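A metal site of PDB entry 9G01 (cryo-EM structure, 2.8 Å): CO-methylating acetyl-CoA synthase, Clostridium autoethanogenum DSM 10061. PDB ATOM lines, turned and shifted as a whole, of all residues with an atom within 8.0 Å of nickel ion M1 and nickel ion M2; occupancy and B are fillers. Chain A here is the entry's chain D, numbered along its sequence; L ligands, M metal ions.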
ATOM      1  N   ARG A 121       6.832 -35.021  15.666  1.00  0.00           N
ATOM      2  CA  ARG A 121       6.841 -33.622  15.252  1.00  0.00           C
ATOM      3  C   ARG A 121       7.816 -32.804  16.086  1.00  0.00           C
ATOM      4  O   ARG A 121       8.379 -31.815  15.584  1.00  0.00           O
ATOM      5  CB  ARG A 121       5.439 -33.041  15.360  1.00  0.00           C
ATOM      6  CG  ARG A 121       4.386 -33.788  14.563  1.00  0.00           C
ATOM      7  CD  ARG A 121       3.014 -33.167  14.736  1.00  0.00           C
ATOM      8  NE  ARG A 121       1.944 -34.013  14.227  1.00  0.00           N
ATOM      9  CZ  ARG A 121       1.452 -33.948  12.993  1.00  0.00           C
ATOM     10  NH1 ARG A 121       1.895 -33.067  12.110  1.00  0.00           N
ATOM     11  NH2 ARG A 121       0.486 -34.795  12.646  1.00  0.00           N
ATOM     12  N   GLY A 124      11.010 -33.288  14.526  1.00  0.00           N
ATOM     13  CA  GLY A 124      11.020 -32.987  13.109  1.00  0.00           C
ATOM     14  C   GLY A 124      11.947 -31.846  12.751  1.00  0.00           C
ATOM     15  O   GLY A 124      12.666 -31.903  11.755  1.00  0.00           O
ATOM     16  N   VAL A 125      11.943 -30.777  13.548  1.00  0.00           N
ATOM     17  CA  VAL A 125      12.820 -29.617  13.328  1.00  0.00           C
ATOM     18  C   VAL A 125      14.283 -30.027  13.429  1.00  0.00           C
ATOM     19  O   VAL A 125      15.064 -29.774  12.507  1.00  0.00           O
ATOM     20  CB  VAL A 125      12.471 -28.458  14.250  1.00  0.00           C
ATOM     21  CG1 VAL A 125      13.582 -27.419  14.237  1.00  0.00           C
ATOM     22  CG2 VAL A 125      11.169 -27.826  13.808  1.00  0.00           C
ATOM     23  N   VAL A 128      15.449 -31.438  10.296  1.00  0.00           N
ATOM     24  CA  VAL A 128      15.604 -30.509   9.158  1.00  0.00           C
ATOM     25  C   VAL A 128      16.787 -29.570   9.356  1.00  0.00           C
ATOM     26  O   VAL A 128      17.500 -29.245   8.401  1.00  0.00           O
ATOM     27  CB  VAL A 128      14.310 -29.720   8.823  1.00  0.00           C
ATOM     28  CG1 VAL A 128      13.214 -30.663   8.369  1.00  0.00           C
ATOM     29  CG2 VAL A 128      13.835 -28.808   9.938  1.00  0.00           C
ATOM     30  N   ILE A 208       3.643 -37.385   7.576  1.00  0.00           N
ATOM     31  CA  ILE A 208       3.471 -36.074   8.207  1.00  0.00           C
ATOM     32  C   ILE A 208       4.176 -34.990   7.405  1.00  0.00           C
ATOM     33  O   ILE A 208       3.547 -34.039   6.930  1.00  0.00           O
ATOM     34  CB  ILE A 208       3.994 -36.108   9.658  1.00  0.00           C
ATOM     35  CG1 ILE A 208       3.094 -37.011  10.519  1.00  0.00           C
ATOM     36  CG2 ILE A 208       4.058 -34.707  10.246  1.00  0.00           C
ATOM     37  CD1 ILE A 208       3.611 -37.246  11.922  1.00  0.00           C
ATOM     38  N   PHE A 209       5.491 -35.113   7.246  1.00  0.00           N
ATOM     39  CA  PHE A 209       6.254 -34.042   6.608  1.00  0.00           C
ATOM     40  C   PHE A 209       6.188 -34.138   5.095  1.00  0.00           C
ATOM     41  O   PHE A 209       6.101 -33.114   4.413  1.00  0.00           O
ATOM     42  CB  PHE A 209       7.707 -34.078   7.077  1.00  0.00           C
ATOM     43  CG  PHE A 209       7.847 -34.068   8.566  1.00  0.00           C
ATOM     44  CD1 PHE A 209       7.490 -32.958   9.303  1.00  0.00           C
ATOM     45  CD2 PHE A 209       8.355 -35.162   9.225  1.00  0.00           C
ATOM     46  CE1 PHE A 209       7.635 -32.940  10.669  1.00  0.00           C
ATOM     47  CE2 PHE A 209       8.504 -35.158  10.592  1.00  0.00           C
ATOM     48  CZ  PHE A 209       8.133 -34.047  11.312  1.00  0.00           C
ATOM     49  N   LEU A 487      13.844 -23.850   4.915  1.00  0.00           N
ATOM     50  CA  LEU A 487      14.655 -24.837   5.625  1.00  0.00           C
ATOM     51  C   LEU A 487      13.921 -26.165   5.727  1.00  0.00           C
ATOM     52  O   LEU A 487      14.538 -27.226   5.570  1.00  0.00           O
ATOM     53  CB  LEU A 487      15.019 -24.302   7.017  1.00  0.00           C
ATOM     54  CG  LEU A 487      15.967 -25.198   7.831  1.00  0.00           C
ATOM     55  CD1 LEU A 487      17.299 -25.430   7.110  1.00  0.00           C
ATOM     56  CD2 LEU A 487      16.199 -24.577   9.200  1.00  0.00           C
ATOM     57  N   CYS A 488      12.625 -26.127   5.979  1.00  0.00           N
ATOM     58  CA  CYS A 488      11.835 -27.351   6.143  1.00  0.00           C
ATOM     59  C   CYS A 488      11.556 -28.066   4.839  1.00  0.00           C
ATOM     60  O   CYS A 488      10.804 -29.041   4.846  1.00  0.00           O
ATOM     61  CB  CYS A 488      10.504 -27.035   6.835  1.00  0.00           C
ATOM     62  SG  CYS A 488      10.629 -26.824   8.629  1.00  0.00           S
ATOM     63  N   GLN A 489      12.131 -27.639   3.715  1.00  0.00           N
ATOM     64  CA  GLN A 489      11.944 -28.330   2.448  1.00  0.00           C
ATOM     65  C   GLN A 489      12.716 -29.634   2.363  1.00  0.00           C
ATOM     66  O   GLN A 489      12.457 -30.431   1.449  1.00  0.00           O
ATOM     67  CB  GLN A 489      12.338 -27.442   1.279  1.00  0.00           C
ATOM     68  CG  GLN A 489      11.275 -26.407   0.913  1.00  0.00           C
ATOM     69  CD  GLN A 489      11.524 -25.764  -0.448  1.00  0.00           C
ATOM     70  OE1 GLN A 489      10.707 -24.975  -0.910  1.00  0.00           O
ATOM     71  NE2 GLN A 489      12.652 -26.101  -1.088  1.00  0.00           N
ATOM     72  N   SER A 490      13.663 -29.865   3.278  1.00  0.00           N
ATOM     73  CA  SER A 490      14.358 -31.151   3.279  1.00  0.00           C
ATOM     74  C   SER A 490      13.421 -32.308   3.586  1.00  0.00           C
ATOM     75  O   SER A 490      13.769 -33.464   3.299  1.00  0.00           O
ATOM     76  CB  SER A 490      15.522 -31.092   4.291  1.00  0.00           C
ATOM     77  OG  SER A 490      16.169 -32.353   4.406  1.00  0.00           O
ATOM     78  N   PHE A 491      12.275 -32.044   4.219  1.00  0.00           N
ATOM     79  CA  PHE A 491      11.272 -33.062   4.491  1.00  0.00           C
ATOM     80  C   PHE A 491       9.895 -32.766   3.916  1.00  0.00           C
ATOM     81  O   PHE A 491       9.124 -33.697   3.684  1.00  0.00           O
ATOM     82  CB  PHE A 491      11.126 -33.314   6.007  1.00  0.00           C
ATOM     83  CG  PHE A 491      12.096 -34.322   6.551  1.00  0.00           C
ATOM     84  CD1 PHE A 491      13.469 -34.166   6.359  1.00  0.00           C
ATOM     85  CD2 PHE A 491      11.636 -35.430   7.267  1.00  0.00           C
ATOM     86  CE1 PHE A 491      14.385 -35.105   6.870  1.00  0.00           C
ATOM     87  CE2 PHE A 491      12.532 -36.389   7.781  1.00  0.00           C
ATOM     88  CZ  PHE A 491      13.914 -36.224   7.588  1.00  0.00           C
ATOM     89  N   ALA A 492       9.576 -31.492   3.644  1.00  0.00           N
ATOM     90  CA  ALA A 492       8.335 -31.068   3.021  1.00  0.00           C
ATOM     91  C   ALA A 492       8.662 -30.255   1.770  1.00  0.00           C
ATOM     92  O   ALA A 492       8.777 -29.021   1.832  1.00  0.00           O
ATOM     93  CB  ALA A 492       7.484 -30.244   3.994  1.00  0.00           C
ATOM     94  N   HIS A 495       6.535 -26.992   0.922  1.00  0.00           N
ATOM     95  CA  HIS A 495       6.254 -26.038   1.988  1.00  0.00           C
ATOM     96  C   HIS A 495       7.266 -24.901   1.974  1.00  0.00           C
ATOM     97  O   HIS A 495       8.482 -25.140   1.989  1.00  0.00           O
ATOM     98  CB  HIS A 495       6.291 -26.734   3.348  1.00  0.00           C
ATOM     99  CG  HIS A 495       6.330 -25.775   4.498  1.00  0.00           C
ATOM    100  ND1 HIS A 495       5.326 -24.876   4.757  1.00  0.00           N
ATOM    101  CD2 HIS A 495       7.273 -25.557   5.450  1.00  0.00           C
ATOM    102  CE1 HIS A 495       5.631 -24.144   5.807  1.00  0.00           C
ATOM    103  NE2 HIS A 495       6.816 -24.548   6.260  1.00  0.00           N
ATOM    104  N   CYS A 497       7.738 -21.087   4.044  1.00  0.00           N
ATOM    105  CA  CYS A 497       7.283 -20.132   5.048  1.00  0.00           C
ATOM    106  C   CYS A 497       7.533 -18.709   4.582  1.00  0.00           C
ATOM    107  O   CYS A 497       8.443 -18.455   3.787  1.00  0.00           O
ATOM    108  CB  CYS A 497       8.005 -20.348   6.382  1.00  0.00           C
ATOM    109  SG  CYS A 497       7.278 -21.639   7.406  1.00  0.00           S
ATOM    110  N   LEU A 506       6.157 -20.974  11.614  1.00  0.00           N
ATOM    111  CA  LEU A 506       5.252 -21.850  12.355  1.00  0.00           C
ATOM    112  C   LEU A 506       6.001 -22.769  13.308  1.00  0.00           C
ATOM    113  O   LEU A 506       5.417 -23.215  14.307  1.00  0.00           O
ATOM    114  CB  LEU A 506       4.372 -22.651  11.390  1.00  0.00           C
ATOM    115  CG  LEU A 506       5.064 -23.537  10.351  1.00  0.00           C
ATOM    116  CD1 LEU A 506       5.023 -25.005  10.757  1.00  0.00           C
ATOM    117  CD2 LEU A 506       4.395 -23.344   9.008  1.00  0.00           C
ATOM    118  N   CYS A 507       7.275 -23.036  13.047  1.00  0.00           N
ATOM    119  CA  CYS A 507       8.079 -23.799  14.001  1.00  0.00           C
ATOM    120  C   CYS A 507       8.331 -23.020  15.290  1.00  0.00           C
ATOM    121  O   CYS A 507       8.609 -23.633  16.322  1.00  0.00           O
ATOM    122  CB  CYS A 507       9.401 -24.229  13.366  1.00  0.00           C
ATOM    123  SG  CYS A 507      10.473 -22.837  12.972  1.00  0.00           S
ATOM    124  N   THR A 572       0.954 -22.823   3.770  1.00  0.00           N
ATOM    125  CA  THR A 572       1.084 -24.229   4.113  1.00  0.00           C
ATOM    126  C   THR A 572       1.921 -24.400   5.382  1.00  0.00           C
ATOM    127  O   THR A 572       2.716 -23.530   5.762  1.00  0.00           O
ATOM    128  CB  THR A 572       1.715 -25.021   2.963  1.00  0.00           C
ATOM    129  OG1 THR A 572       2.988 -24.471   2.608  1.00  0.00           O
ATOM    130  CG2 THR A 572       0.819 -24.994   1.750  1.00  0.00           C
ATOM    131  N   SER A 573       1.730 -25.544   6.036  1.00  0.00           N
ATOM    132  CA  SER A 573       2.539 -25.979   7.155  1.00  0.00           C
ATOM    133  C   SER A 573       3.082 -27.351   6.832  1.00  0.00           C
ATOM    134  O   SER A 573       2.582 -28.029   5.927  1.00  0.00           O
ATOM    135  CB  SER A 573       1.728 -26.053   8.473  1.00  0.00           C
ATOM    136  OG  SER A 573       1.086 -24.816   8.775  1.00  0.00           O
ATOM    137  N   CYS A 574       4.127 -27.789   7.546  1.00  0.00           N
ATOM    138  CA  CYS A 574       4.771 -29.049   7.235  1.00  0.00           C
ATOM    139  C   CYS A 574       4.481 -30.048   8.349  1.00  0.00           C
ATOM    140  O   CYS A 574       3.701 -30.987   8.135  1.00  0.00           O
ATOM    141  CB  CYS A 574       6.278 -28.825   7.051  1.00  0.00           C
ATOM    142  SG  CYS A 574       6.921 -27.637   8.245  1.00  0.00           S
ATOM    143  N   GLY A 575       5.098 -29.916   9.514  1.00  0.00           N
ATOM    144  CA  GLY A 575       4.733 -30.781  10.627  1.00  0.00           C
ATOM    145  C   GLY A 575       5.100 -30.235  11.988  1.00  0.00           C
ATOM    146  O   GLY A 575       4.899 -30.895  13.007  1.00  0.00           O
ATOM    147  N   CYS A 576       5.629 -29.013  12.025  1.00  0.00           N
ATOM    148  CA  CYS A 576       6.370 -28.508  13.172  1.00  0.00           C
ATOM    149  C   CYS A 576       5.678 -27.368  13.902  1.00  0.00           C
ATOM    150  O   CYS A 576       6.255 -26.784  14.819  1.00  0.00           O
ATOM    151  CB  CYS A 576       7.764 -28.063  12.713  1.00  0.00           C
ATOM    152  SG  CYS A 576       7.695 -27.023  11.231  1.00  0.00           S
ATOM    153  N   PHE A 577       4.438 -27.058  13.527  1.00  0.00           N
ATOM    154  CA  PHE A 577       3.733 -25.949  14.163  1.00  0.00           C
ATOM    155  C   PHE A 577       3.517 -26.218  15.641  1.00  0.00           C
ATOM    156  O   PHE A 577       3.138 -27.326  16.030  1.00  0.00           O
ATOM    157  CB  PHE A 577       2.399 -25.696  13.453  1.00  0.00           C
ATOM    158  CG  PHE A 577       1.708 -26.939  12.995  1.00  0.00           C
ATOM    159  CD1 PHE A 577       0.891 -27.655  13.853  1.00  0.00           C
ATOM    160  CD2 PHE A 577       1.905 -27.414  11.694  1.00  0.00           C
ATOM    161  CE1 PHE A 577       0.252 -28.834  13.432  1.00  0.00           C
ATOM    162  CE2 PHE A 577       1.286 -28.575  11.254  1.00  0.00           C
ATOM    163  CZ  PHE A 577       0.453 -29.295  12.118  1.00  0.00           C
ATOM    164  N   GLU A 578       3.797 -25.206  16.461  1.00  0.00           N
ATOM    165  CA  GLU A 578       3.604 -25.333  17.902  1.00  0.00           C
ATOM    166  C   GLU A 578       2.135 -25.510  18.249  1.00  0.00           C
ATOM    167  O   GLU A 578       1.783 -26.349  19.085  1.00  0.00           O
ATOM    168  CB  GLU A 578       4.170 -24.100  18.608  1.00  0.00           C
ATOM    169  CG  GLU A 578       5.658 -23.896  18.367  1.00  0.00           C
ATOM    170  CD  GLU A 578       6.141 -22.596  18.971  1.00  0.00           C
ATOM    171  OE1 GLU A 578       5.313 -21.678  19.109  1.00  0.00           O
ATOM    172  OE2 GLU A 578       7.336 -22.484  19.329  1.00  0.00           O
ATOM    173  N   ARG A 595       0.926 -28.509  20.858  1.00  0.00           N
ATOM    174  CA  ARG A 595       1.445 -29.867  20.749  1.00  0.00           C
ATOM    175  C   ARG A 595       1.507 -30.547  22.118  1.00  0.00           C
ATOM    176  O   ARG A 595       1.264 -31.749  22.227  1.00  0.00           O
ATOM    177  CB  ARG A 595       2.818 -29.871  20.084  1.00  0.00           C
ATOM    178  CG  ARG A 595       3.433 -31.278  20.009  1.00  0.00           C
ATOM    179  CD  ARG A 595       4.308 -31.466  18.762  1.00  0.00           C
ATOM    180  NE  ARG A 595       5.519 -30.658  18.802  1.00  0.00           N
ATOM    181  CZ  ARG A 595       5.775 -29.614  18.033  1.00  0.00           C
ATOM    182  NH1 ARG A 595       4.929 -29.216  17.100  1.00  0.00           N
ATOM    183  NH2 ARG A 595       6.929 -28.965  18.172  1.00  0.00           N
ATOM    184  N   THR A 614      -3.415 -30.783   8.157  1.00  0.00           N
ATOM    185  CA  THR A 614      -2.941 -29.554   7.541  1.00  0.00           C
ATOM    186  C   THR A 614      -1.435 -29.540   7.286  1.00  0.00           C
ATOM    187  O   THR A 614      -0.863 -28.455   7.149  1.00  0.00           O
ATOM    188  CB  THR A 614      -3.319 -28.344   8.404  1.00  0.00           C
ATOM    189  OG1 THR A 614      -2.892 -27.130   7.772  1.00  0.00           O
ATOM    190  CG2 THR A 614      -2.672 -28.442   9.781  1.00  0.00           C
ATOM    191  N   GLY A 615      -0.784 -30.695   7.188  1.00  0.00           N
ATOM    192  CA  GLY A 615       0.647 -30.763   7.032  1.00  0.00           C
ATOM    193  C   GLY A 615       1.085 -31.276   5.659  1.00  0.00           C
ATOM    194  O   GLY A 615       0.286 -31.603   4.796  1.00  0.00           O
ATOM    195  N   GLY A 616       2.403 -31.332   5.497  1.00  0.00           N
ATOM    196  CA  GLY A 616       3.006 -31.864   4.299  1.00  0.00           C
ATOM    197  C   GLY A 616       3.137 -30.894   3.139  1.00  0.00           C
ATOM    198  O   GLY A 616       3.546 -31.316   2.057  1.00  0.00           O
ATOM    199  N   GLY A 617       2.820 -29.623   3.335  1.00  0.00           N
ATOM    200  CA  GLY A 617       2.901 -28.664   2.252  1.00  0.00           C
ATOM    201  C   GLY A 617       1.683 -28.579   1.372  1.00  0.00           C
ATOM    202  O   GLY A 617       1.789 -28.101   0.239  1.00  0.00           O
HETATM  203  C1  LIG L   1       9.639 -29.594   9.514  1.00  0.00           C
HETATM  204  O1  LIG L   1      10.154 -30.719   9.600  1.00  0.00           O
HETATM  205 FE1  LG2 L   2      11.909 -22.400   8.527  1.00  0.00          FE
HETATM  206 FE2  LG2 L   2       9.196 -22.512   8.230  1.00  0.00          FE
HETATM  207 FE3  LG2 L   2      10.303 -22.700  10.717  1.00  0.00          FE
HETATM  208 FE4  LG2 L   2      10.584 -24.758   8.934  1.00  0.00          FE
HETATM  209  S1  LG2 L   2       8.643 -24.005   9.857  1.00  0.00           S
HETATM  210  S2  LG2 L   2      12.209 -23.860  10.258  1.00  0.00           S
HETATM  211  S3  LG2 L   2      10.758 -23.609   6.974  1.00  0.00           S
HETATM  212  S4  LG2 L   2      10.393 -20.906   9.327  1.00  0.00           S
HETATM  213 NI    NI M   1       8.951 -28.122   9.400  1.00  0.00          NI
HETATM  214 NI    NI M   2       6.272 -28.470  10.248  1.00  0.00          NI
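Residues that only touch nickel ion M2: Leu 506 (3.7 Å). The nearest printed residue that does not touch nickel ion M2 is Phe 577 (4.01 Å).
A sulfur (S3) of LG2 L2 lies close to the backbone NH (N) of Cys 488, 3.3 Å away. The side-chain sulfur (SG) of Cys 507 binds an iron atom (FE3) of LG2 L2, at 2.3 Å. S1 of LG2 L2 lies close to N of Cys 507. SG of Cys 497 is bound to FE2 of LG2 L2 (2.3 Å). The backbone NH of Leu 487 sits close to a sulfur (S3) of LG2 L2 (3.7 Å). FE4 of LG2 L2 is bound by SG of Cys 488, 2.1 Å away.
Within 4 Å of nickel ion M1: Cys 488, Cys 574 and Cys 576. The nearest printed residue that does not touch nickel ion M1 is Gly 575 (4.3 Å).
Nickel ion M1 is bound by SG of Cys 488 (2.3 Å). SG of Cys 574 is bound to nickel ion M1. SG of Cys 576 is bound to nickel ion M1 (2.5 Å).
Nickel ion M2 is bound by N of Cys 576 (2.0 Å), N of Gly 575 (2.0 Å), SG of Cys 576 (2.3 Å) and SG of Cys 574 (2.3 Å).
The backbone NH (N) of Glu 578 is in hydrogen-bond range of the backbone carbonyl oxygen (O) of Leu 506, 3.4 Å away. The backbone NH (N) of Gly 616 is in hydrogen-bond range of the backbone carbonyl oxygen (O) of Cys 574, at 3.0 Å. A ring nitrogen (NE2) of His 495 lies close to the side-chain sulfur (SG) of Cys 574.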
